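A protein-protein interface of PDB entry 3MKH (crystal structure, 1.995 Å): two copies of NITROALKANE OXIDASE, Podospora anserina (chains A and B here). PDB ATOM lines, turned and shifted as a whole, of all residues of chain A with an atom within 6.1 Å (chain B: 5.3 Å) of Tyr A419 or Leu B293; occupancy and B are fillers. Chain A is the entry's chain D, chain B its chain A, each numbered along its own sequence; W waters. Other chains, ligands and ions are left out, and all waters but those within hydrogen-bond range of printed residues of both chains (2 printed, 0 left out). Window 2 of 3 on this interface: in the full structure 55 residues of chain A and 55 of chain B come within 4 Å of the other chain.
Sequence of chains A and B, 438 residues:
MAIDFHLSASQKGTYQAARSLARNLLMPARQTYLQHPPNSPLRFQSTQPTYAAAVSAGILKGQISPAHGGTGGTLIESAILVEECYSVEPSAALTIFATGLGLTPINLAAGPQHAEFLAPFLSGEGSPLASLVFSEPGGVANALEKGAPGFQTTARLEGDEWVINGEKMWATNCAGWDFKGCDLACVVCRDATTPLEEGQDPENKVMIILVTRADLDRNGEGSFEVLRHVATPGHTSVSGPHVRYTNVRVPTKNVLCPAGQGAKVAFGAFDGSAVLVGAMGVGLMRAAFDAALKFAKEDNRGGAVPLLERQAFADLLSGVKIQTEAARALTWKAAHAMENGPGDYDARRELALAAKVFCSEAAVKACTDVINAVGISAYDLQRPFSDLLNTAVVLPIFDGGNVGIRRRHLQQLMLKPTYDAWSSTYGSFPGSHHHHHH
The side-chain carboxylate (OE2) of Glu A350 lies within hydrogen-bond range of the side-chain hydroxyl (OH) of Tyr A419 (2.5 Å).
NZ of Lys B321 lies within salt-bridge range of OE1 of Glu A350. The backbone carbonyl oxygen of Met A414 is in hydrogen-bond range of the side-chain amino group of Lys B297, 2.8 Å away. OD1 of Asp B290 lies within hydrogen-bond range of NE1 of Trp A422, at 2.9 Å. The side-chain amino group (NZ) of Lys B321 is in hydrogen-bond range of the backbone carbonyl oxygen (O) of Ala A421 (3.0 Å). The backbone carbonyl oxygen of Lys A416 is in hydrogen-bond range of the side-chain amino group of Lys B297 (3.3 Å).
Water W2 bridges O of Leu A415 and NZ of Lys B297. Water W1 lies within hydrogen-bond range of the backbone carbonyl oxygen of Tyr A419 (2.8 Å) and the side-chain amino group of Lys B297 (2.9 Å).
Printed residues of chain B that touch a printed residue of chain A: Phe B289, Asp B290, Leu B293, Lys B297, Leu B308 and Lys B321. Hydrophobic or aromatic side chains of chain B within 4 Å of the printed part of chain A: Phe B289, Leu B293 and Leu B308. Printed residues of chain A that touch a printed residue of chain B: Glu A350, Met A414, Leu A415, Lys A416, Tyr A419, Ala A421 and Trp A422. Hydrophobic or aromatic side chains of chain A that line the printed part of chain B: Leu A415, Tyr A419, Ala A421 and Trp A422.
No position is printed for both chains. Of the 13 pairs that touch across the chains among the printed residues, none has its exchanged pair printed and touching as well.
Tyr A419 touches three residues of chain B. Of chain A, only Tyr A419 comes within 4 Å of Leu B293. Of the printed residues of chain B, Glu A350 touches Lys B321 (2.8 Å). Of the printed residues of chain A, Phe B289 touches Tyr A419, Ala A421 and Trp A422. Printed residues of chain A within 4 Å of Lys B321: Glu A350 (2.8 Å), Tyr A419 (3.4 Å), Ala A421 (3.0 Å) and Trp A422 (3.5 Å). Asp A420 touches none of the printed residues of chain B. The nearest residue of chain A that does not touch Leu B293 is Ala A421 (4.8 Å).
Among the printed residues, pairs that only touch across the chains: Leu A415 with Leu B308, Tyr A419 with Lys B321, Trp A422 with Lys B321, Tyr A419 with Phe B289, Met A414 with Leu B308, Tyr A419 with Leu B293, Ala A421 with Phe B289 and Trp A422 with Phe B289.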
ATOM      1  N   GLU A 350     -24.352  -3.158   7.362  1.00  0.00           N
ATOM      2  CA  GLU A 350     -23.493  -2.532   6.363  1.00  0.00           C
ATOM      3  C   GLU A 350     -22.799  -3.639   5.600  1.00  0.00           C
ATOM      4  O   GLU A 350     -22.640  -3.569   4.378  1.00  0.00           O
ATOM      5  CB  GLU A 350     -22.461  -1.594   6.991  1.00  0.00           C
ATOM      6  CG  GLU A 350     -21.626  -0.850   5.934  1.00  0.00           C
ATOM      7  CD  GLU A 350     -20.345  -0.239   6.488  1.00  0.00           C
ATOM      8  OE1 GLU A 350     -19.554  -0.969   7.124  1.00  0.00           O
ATOM      9  OE2 GLU A 350     -20.110   0.967   6.261  1.00  0.00           O
ATOM     10  N   LEU A 410     -26.694   2.655   2.909  1.00  0.00           N
ATOM     11  CA  LEU A 410     -25.276   2.745   3.265  1.00  0.00           C
ATOM     12  C   LEU A 410     -24.925   4.183   3.615  1.00  0.00           C
ATOM     13  O   LEU A 410     -24.183   4.447   4.554  1.00  0.00           O
ATOM     14  CB  LEU A 410     -24.394   2.264   2.118  1.00  0.00           C
ATOM     15  CG  LEU A 410     -24.423   0.766   1.863  1.00  0.00           C
ATOM     16  CD1 LEU A 410     -23.730   0.445   0.543  1.00  0.00           C
ATOM     17  CD2 LEU A 410     -23.771   0.031   3.023  1.00  0.00           C
ATOM     18  N   LEU A 413     -26.312   4.984   7.061  1.00  0.00           N
ATOM     19  CA  LEU A 413     -25.492   4.326   8.072  1.00  0.00           C
ATOM     20  C   LEU A 413     -24.291   5.187   8.401  1.00  0.00           C
ATOM     21  O   LEU A 413     -24.010   5.463   9.569  1.00  0.00           O
ATOM     22  CB  LEU A 413     -25.010   2.955   7.578  1.00  0.00           C
ATOM     23  CG  LEU A 413     -26.072   1.868   7.586  1.00  0.00           C
ATOM     24  CD1 LEU A 413     -25.569   0.626   6.883  1.00  0.00           C
ATOM     25  CD2 LEU A 413     -26.491   1.565   9.019  1.00  0.00           C
ATOM     26  N   MET A 414     -23.586   5.615   7.357  1.00  0.00           N
ATOM     27  CA  MET A 414     -22.342   6.364   7.528  1.00  0.00           C
ATOM     28  C   MET A 414     -22.591   7.749   8.115  1.00  0.00           C
ATOM     29  O   MET A 414     -21.706   8.331   8.723  1.00  0.00           O
ATOM     30  CB  MET A 414     -21.597   6.509   6.197  1.00  0.00           C
ATOM     31  CG  MET A 414     -21.032   5.223   5.594  1.00  0.00           C
ATOM     32  SD  MET A 414     -20.046   5.577   4.108  1.00  0.00           S
ATOM     33  CE  MET A 414     -21.338   5.895   2.907  1.00  0.00           C
ATOM     34  N   LEU A 415     -23.789   8.287   7.911  1.00  0.00           N
ATOM     35  CA  LEU A 415     -24.119   9.624   8.407  1.00  0.00           C
ATOM     36  C   LEU A 415     -24.365   9.660   9.919  1.00  0.00           C
ATOM     37  O   LEU A 415     -24.268  10.712  10.547  1.00  0.00           O
ATOM     38  CB  LEU A 415     -25.347  10.168   7.679  1.00  0.00           C
ATOM     39  CG  LEU A 415     -25.112  10.938   6.378  1.00  0.00           C
ATOM     40  CD1 LEU A 415     -26.418  11.094   5.619  1.00  0.00           C
ATOM     41  CD2 LEU A 415     -24.493  12.291   6.689  1.00  0.00           C
ATOM     42  N   LYS A 416     -24.699   8.514  10.499  1.00  0.00           N
ATOM     43  CA  LYS A 416     -24.949   8.445  11.936  1.00  0.00           C
ATOM     44  C   LYS A 416     -23.694   8.777  12.745  1.00  0.00           C
ATOM     45  O   LYS A 416     -22.599   8.310  12.430  1.00  0.00           O
ATOM     46  CB  LYS A 416     -25.467   7.069  12.315  1.00  0.00           C
ATOM     47  CG  LYS A 416     -26.808   6.723  11.695  1.00  0.00           C
ATOM     48  CD  LYS A 416     -27.439   5.547  12.405  1.00  0.00           C
ATOM     49  CE  LYS A 416     -28.727   5.133  11.722  1.00  0.00           C
ATOM     50  NZ  LYS A 416     -29.365   3.989  12.426  1.00  0.00           N
ATOM     51  N   PRO A 417     -23.851   9.595  13.793  1.00  0.00           N
ATOM     52  CA  PRO A 417     -22.706   9.977  14.626  1.00  0.00           C
ATOM     53  C   PRO A 417     -22.114   8.756  15.316  1.00  0.00           C
ATOM     54  O   PRO A 417     -20.968   8.792  15.748  1.00  0.00           O
ATOM     55  CB  PRO A 417     -23.324  10.922  15.663  1.00  0.00           C
ATOM     56  CG  PRO A 417     -24.587  11.420  15.017  1.00  0.00           C
ATOM     57  CD  PRO A 417     -25.093  10.261  14.220  1.00  0.00           C
ATOM     58  N   THR A 418     -22.887   7.682  15.407  1.00  0.00           N
ATOM     59  CA  THR A 418     -22.406   6.467  16.050  1.00  0.00           C
ATOM     60  C   THR A 418     -21.686   5.517  15.090  1.00  0.00           C
ATOM     61  O   THR A 418     -21.184   4.481  15.513  1.00  0.00           O
ATOM     62  CB  THR A 418     -23.541   5.709  16.760  1.00  0.00           C
ATOM     63  OG1 THR A 418     -24.603   5.454  15.835  1.00  0.00           O
ATOM     64  CG2 THR A 418     -24.072   6.527  17.935  1.00  0.00           C
ATOM     65  N   TYR A 419     -21.639   5.865  13.808  1.00  0.00           N
ATOM     66  CA  TYR A 419     -20.950   5.031  12.822  1.00  0.00           C
ATOM     67  C   TYR A 419     -19.523   4.753  13.290  1.00  0.00           C
ATOM     68  O   TYR A 419     -18.801   5.672  13.695  1.00  0.00           O
ATOM     69  CB  TYR A 419     -20.942   5.717  11.446  1.00  0.00           C
ATOM     70  CG  TYR A 419     -20.305   4.890  10.345  1.00  0.00           C
ATOM     71  CD1 TYR A 419     -20.928   3.747   9.854  1.00  0.00           C
ATOM     72  CD2 TYR A 419     -19.086   5.262   9.793  1.00  0.00           C
ATOM     73  CE1 TYR A 419     -20.347   2.983   8.852  1.00  0.00           C
ATOM     74  CE2 TYR A 419     -18.492   4.508   8.783  1.00  0.00           C
ATOM     75  CZ  TYR A 419     -19.132   3.378   8.309  1.00  0.00           C
ATOM     76  OH  TYR A 419     -18.541   2.634   7.308  1.00  0.00           O
ATOM     77  N   ASP A 420     -19.131   3.483  13.249  1.00  0.00           N
ATOM     78  CA  ASP A 420     -17.807   3.060  13.697  1.00  0.00           C
ATOM     79  C   ASP A 420     -17.260   2.108  12.646  1.00  0.00           C
ATOM     80  O   ASP A 420     -17.520   0.904  12.688  1.00  0.00           O
ATOM     81  CB  ASP A 420     -17.893   2.371  15.067  1.00  0.00           C
ATOM     82  CG  ASP A 420     -16.521   2.112  15.689  1.00  0.00           C
ATOM     83  OD1 ASP A 420     -15.498   2.451  15.064  1.00  0.00           O
ATOM     84  OD2 ASP A 420     -16.463   1.578  16.816  1.00  0.00           O
ATOM     85  N   ALA A 421     -16.492   2.659  11.709  1.00  0.00           N
ATOM     86  CA  ALA A 421     -16.186   1.971  10.449  1.00  0.00           C
ATOM     87  C   ALA A 421     -15.819   0.493  10.562  1.00  0.00           C
ATOM     88  O   ALA A 421     -16.419  -0.349   9.888  1.00  0.00           O
ATOM     89  CB  ALA A 421     -15.105   2.732   9.679  1.00  0.00           C
ATOM     90  N   TRP A 422     -14.833   0.165  11.392  1.00  0.00           N
ATOM     91  CA  TRP A 422     -14.293  -1.191  11.371  1.00  0.00           C
ATOM     92  C   TRP A 422     -14.763  -2.057  12.545  1.00  0.00           C
ATOM     93  O   TRP A 422     -14.227  -3.146  12.774  1.00  0.00           O
ATOM     94  CB  TRP A 422     -12.762  -1.145  11.288  1.00  0.00           C
ATOM     95  CG  TRP A 422     -12.344  -0.150  10.265  1.00  0.00           C
ATOM     96  CD1 TRP A 422     -11.838   1.101  10.489  1.00  0.00           C
ATOM     97  CD2 TRP A 422     -12.483  -0.283   8.848  1.00  0.00           C
ATOM     98  NE1 TRP A 422     -11.608   1.739   9.290  1.00  0.00           N
ATOM     99  CE2 TRP A 422     -11.996   0.913   8.267  1.00  0.00           C
ATOM    100  CE3 TRP A 422     -12.934  -1.313   8.008  1.00  0.00           C
ATOM    101  CZ2 TRP A 422     -11.967   1.114   6.887  1.00  0.00           C
ATOM    102  CZ3 TRP A 422     -12.901  -1.117   6.638  1.00  0.00           C
ATOM    103  CH2 TRP A 422     -12.423   0.093   6.089  1.00  0.00           C
ATOM    104  N   ALA B 288      -7.230   5.250   3.511  1.00  0.00           N
ATOM    105  CA  ALA B 288      -7.846   6.169   2.557  1.00  0.00           C
ATOM    106  C   ALA B 288      -9.305   6.419   2.934  1.00  0.00           C
ATOM    107  O   ALA B 288      -9.774   7.566   2.945  1.00  0.00           O
ATOM    108  CB  ALA B 288      -7.736   5.617   1.133  1.00  0.00           C
ATOM    109  N   PHE B 289     -10.020   5.343   3.257  1.00  0.00           N
ATOM    110  CA  PHE B 289     -11.409   5.475   3.691  1.00  0.00           C
ATOM    111  C   PHE B 289     -11.510   6.356   4.940  1.00  0.00           C
ATOM    112  O   PHE B 289     -12.325   7.274   4.996  1.00  0.00           O
ATOM    113  CB  PHE B 289     -12.031   4.108   3.972  1.00  0.00           C
ATOM    114  CG  PHE B 289     -13.434   4.193   4.493  1.00  0.00           C
ATOM    115  CD1 PHE B 289     -14.515   4.219   3.618  1.00  0.00           C
ATOM    116  CD2 PHE B 289     -13.675   4.281   5.853  1.00  0.00           C
ATOM    117  CE1 PHE B 289     -15.822   4.314   4.100  1.00  0.00           C
ATOM    118  CE2 PHE B 289     -14.966   4.379   6.344  1.00  0.00           C
ATOM    119  CZ  PHE B 289     -16.046   4.394   5.461  1.00  0.00           C
ATOM    120  N   ASP B 290     -10.687   6.072   5.945  1.00  0.00           N
ATOM    121  CA  ASP B 290     -10.701   6.846   7.186  1.00  0.00           C
ATOM    122  C   ASP B 290     -10.415   8.325   6.977  1.00  0.00           C
ATOM    123  O   ASP B 290     -11.071   9.175   7.583  1.00  0.00           O
ATOM    124  CB  ASP B 290      -9.686   6.289   8.182  1.00  0.00           C
ATOM    125  CG  ASP B 290     -10.144   4.974   8.828  1.00  0.00           C
ATOM    126  OD1 ASP B 290     -11.301   4.548   8.626  1.00  0.00           O
ATOM    127  OD2 ASP B 290      -9.329   4.370   9.547  1.00  0.00           O
ATOM    128  N   ALA B 291      -9.418   8.633   6.151  1.00  0.00           N
ATOM    129  CA  ALA B 291      -9.056  10.030   5.905  1.00  0.00           C
ATOM    130  C   ALA B 291     -10.162  10.793   5.154  1.00  0.00           C
ATOM    131  O   ALA B 291     -10.436  11.956   5.448  1.00  0.00           O
ATOM    132  CB  ALA B 291      -7.726  10.115   5.161  1.00  0.00           C
ATOM    133  N   ALA B 292     -10.801  10.133   4.199  1.00  0.00           N
ATOM    134  CA  ALA B 292     -11.915  10.745   3.461  1.00  0.00           C
ATOM    135  C   ALA B 292     -13.152  10.945   4.345  1.00  0.00           C
ATOM    136  O   ALA B 292     -13.822  11.986   4.274  1.00  0.00           O
ATOM    137  CB  ALA B 292     -12.268   9.909   2.222  1.00  0.00           C
ATOM    138  N   LEU B 293     -13.451   9.950   5.173  1.00  0.00           N
ATOM    139  CA  LEU B 293     -14.578  10.035   6.100  1.00  0.00           C
ATOM    140  C   LEU B 293     -14.338  11.157   7.102  1.00  0.00           C
ATOM    141  O   LEU B 293     -15.242  11.922   7.419  1.00  0.00           O
ATOM    142  CB  LEU B 293     -14.790   8.700   6.831  1.00  0.00           C
ATOM    143  CG  LEU B 293     -16.058   8.558   7.680  1.00  0.00           C
ATOM    144  CD1 LEU B 293     -17.293   8.590   6.802  1.00  0.00           C
ATOM    145  CD2 LEU B 293     -16.015   7.247   8.460  1.00  0.00           C
ATOM    146  N   LYS B 294     -13.107  11.266   7.585  1.00  0.00           N
ATOM    147  CA  LYS B 294     -12.733  12.340   8.497  1.00  0.00           C
ATOM    148  C   LYS B 294     -12.945  13.714   7.849  1.00  0.00           C
ATOM    149  O   LYS B 294     -13.522  14.621   8.449  1.00  0.00           O
ATOM    150  CB  LYS B 294     -11.273  12.183   8.918  1.00  0.00           C
ATOM    151  CG  LYS B 294     -10.800  13.183   9.977  1.00  0.00           C
ATOM    152  CD  LYS B 294      -9.441  12.743  10.539  1.00  0.00           C
ATOM    153  CE  LYS B 294      -9.112  13.421  11.870  1.00  0.00           C
ATOM    154  NZ  LYS B 294      -8.929  14.889  11.723  1.00  0.00           N
ATOM    155  N   PHE B 295     -12.460  13.859   6.623  1.00  0.00           N
ATOM    156  CA  PHE B 295     -12.635  15.083   5.854  1.00  0.00           C
ATOM    157  C   PHE B 295     -14.126  15.390   5.682  1.00  0.00           C
ATOM    158  O   PHE B 295     -14.565  16.511   5.901  1.00  0.00           O
ATOM    159  CB  PHE B 295     -11.914  14.933   4.507  1.00  0.00           C
ATOM    160  CG  PHE B 295     -12.093  16.090   3.564  1.00  0.00           C
ATOM    161  CD1 PHE B 295     -13.123  16.088   2.634  1.00  0.00           C
ATOM    162  CD2 PHE B 295     -11.210  17.146   3.574  1.00  0.00           C
ATOM    163  CE1 PHE B 295     -13.286  17.139   1.746  1.00  0.00           C
ATOM    164  CE2 PHE B 295     -11.358  18.198   2.694  1.00  0.00           C
ATOM    165  CZ  PHE B 295     -12.397  18.191   1.773  1.00  0.00           C
ATOM    166  N   ALA B 296     -14.914  14.382   5.332  1.00  0.00           N
ATOM    167  CA  ALA B 296     -16.346  14.584   5.125  1.00  0.00           C
ATOM    168  C   ALA B 296     -17.084  14.986   6.400  1.00  0.00           C
ATOM    169  O   ALA B 296     -17.991  15.830   6.370  1.00  0.00           O
ATOM    170  CB  ALA B 296     -16.980  13.344   4.538  1.00  0.00           C
ATOM    171  N   LYS B 297     -16.721  14.364   7.517  1.00  0.00           N
ATOM    172  CA  LYS B 297     -17.446  14.627   8.759  1.00  0.00           C
ATOM    173  C   LYS B 297     -17.103  15.994   9.355  1.00  0.00           C
ATOM    174  O   LYS B 297     -17.837  16.511  10.197  1.00  0.00           O
ATOM    175  CB  LYS B 297     -17.267  13.482   9.765  1.00  0.00           C
ATOM    176  CG  LYS B 297     -18.010  12.189   9.336  1.00  0.00           C
ATOM    177  CD  LYS B 297     -18.016  11.089  10.414  1.00  0.00           C
ATOM    178  CE  LYS B 297     -18.810   9.840   9.963  1.00  0.00           C
ATOM    179  NZ  LYS B 297     -20.158   9.645  10.627  1.00  0.00           N
ATOM    180  N   GLU B 298     -16.018  16.605   8.891  1.00  0.00           N
ATOM    181  CA  GLU B 298     -15.631  17.909   9.419  1.00  0.00           C
ATOM    182  C   GLU B 298     -15.661  19.036   8.373  1.00  0.00           C
ATOM    183  O   GLU B 298     -15.407  20.192   8.703  1.00  0.00           O
ATOM    184  CB  GLU B 298     -14.250  17.834  10.060  1.00  0.00           C
ATOM    185  CG  GLU B 298     -13.107  17.982   9.075  1.00  0.00           C
ATOM    186  CD  GLU B 298     -11.732  17.826   9.727  1.00  0.00           C
ATOM    187  OE1 GLU B 298     -11.602  17.062  10.715  1.00  0.00           O
ATOM    188  OE2 GLU B 298     -10.776  18.469   9.238  1.00  0.00           O
ATOM    189  N   LEU B 308     -21.479  14.236   3.554  1.00  0.00           N
ATOM    190  CA  LEU B 308     -21.996  12.876   3.387  1.00  0.00           C
ATOM    191  C   LEU B 308     -23.429  12.824   2.845  1.00  0.00           C
ATOM    192  O   LEU B 308     -23.898  11.764   2.424  1.00  0.00           O
ATOM    193  CB  LEU B 308     -21.864  12.050   4.673  1.00  0.00           C
ATOM    194  CG  LEU B 308     -20.570  11.239   4.837  1.00  0.00           C
ATOM    195  CD1 LEU B 308     -20.530  10.560   6.195  1.00  0.00           C
ATOM    196  CD2 LEU B 308     -20.403  10.220   3.707  1.00  0.00           C
ATOM    197  N   LEU B 317     -17.493   6.813  -1.292  1.00  0.00           N
ATOM    198  CA  LEU B 317     -16.976   6.262  -0.037  1.00  0.00           C
ATOM    199  C   LEU B 317     -17.485   4.854   0.273  1.00  0.00           C
ATOM    200  O   LEU B 317     -16.714   3.995   0.703  1.00  0.00           O
ATOM    201  CB  LEU B 317     -17.299   7.165   1.146  1.00  0.00           C
ATOM    202  CG  LEU B 317     -16.179   8.094   1.578  1.00  0.00           C
ATOM    203  CD1 LEU B 317     -16.554   8.789   2.874  1.00  0.00           C
ATOM    204  CD2 LEU B 317     -14.911   7.282   1.751  1.00  0.00           C
ATOM    205  N   LYS B 321     -15.496   1.377   0.920  1.00  0.00           N
ATOM    206  CA  LYS B 321     -15.736   0.517   2.091  1.00  0.00           C
ATOM    207  C   LYS B 321     -16.042  -0.929   1.673  1.00  0.00           C
ATOM    208  O   LYS B 321     -15.522  -1.896   2.239  1.00  0.00           O
ATOM    209  CB  LYS B 321     -16.878   1.080   2.944  1.00  0.00           C
ATOM    210  CG  LYS B 321     -17.073   0.388   4.305  1.00  0.00           C
ATOM    211  CD  LYS B 321     -15.825   0.462   5.149  1.00  0.00           C
ATOM    212  CE  LYS B 321     -16.151   0.360   6.634  1.00  0.00           C
ATOM    213  NZ  LYS B 321     -16.786  -0.944   7.000  1.00  0.00           N
HETATM  214  O   HOH W   1     -18.915   8.330  12.860  1.00  0.00           O
HETATM  215  O   HOH W   2     -21.867  11.954  10.659  1.00  0.00           O
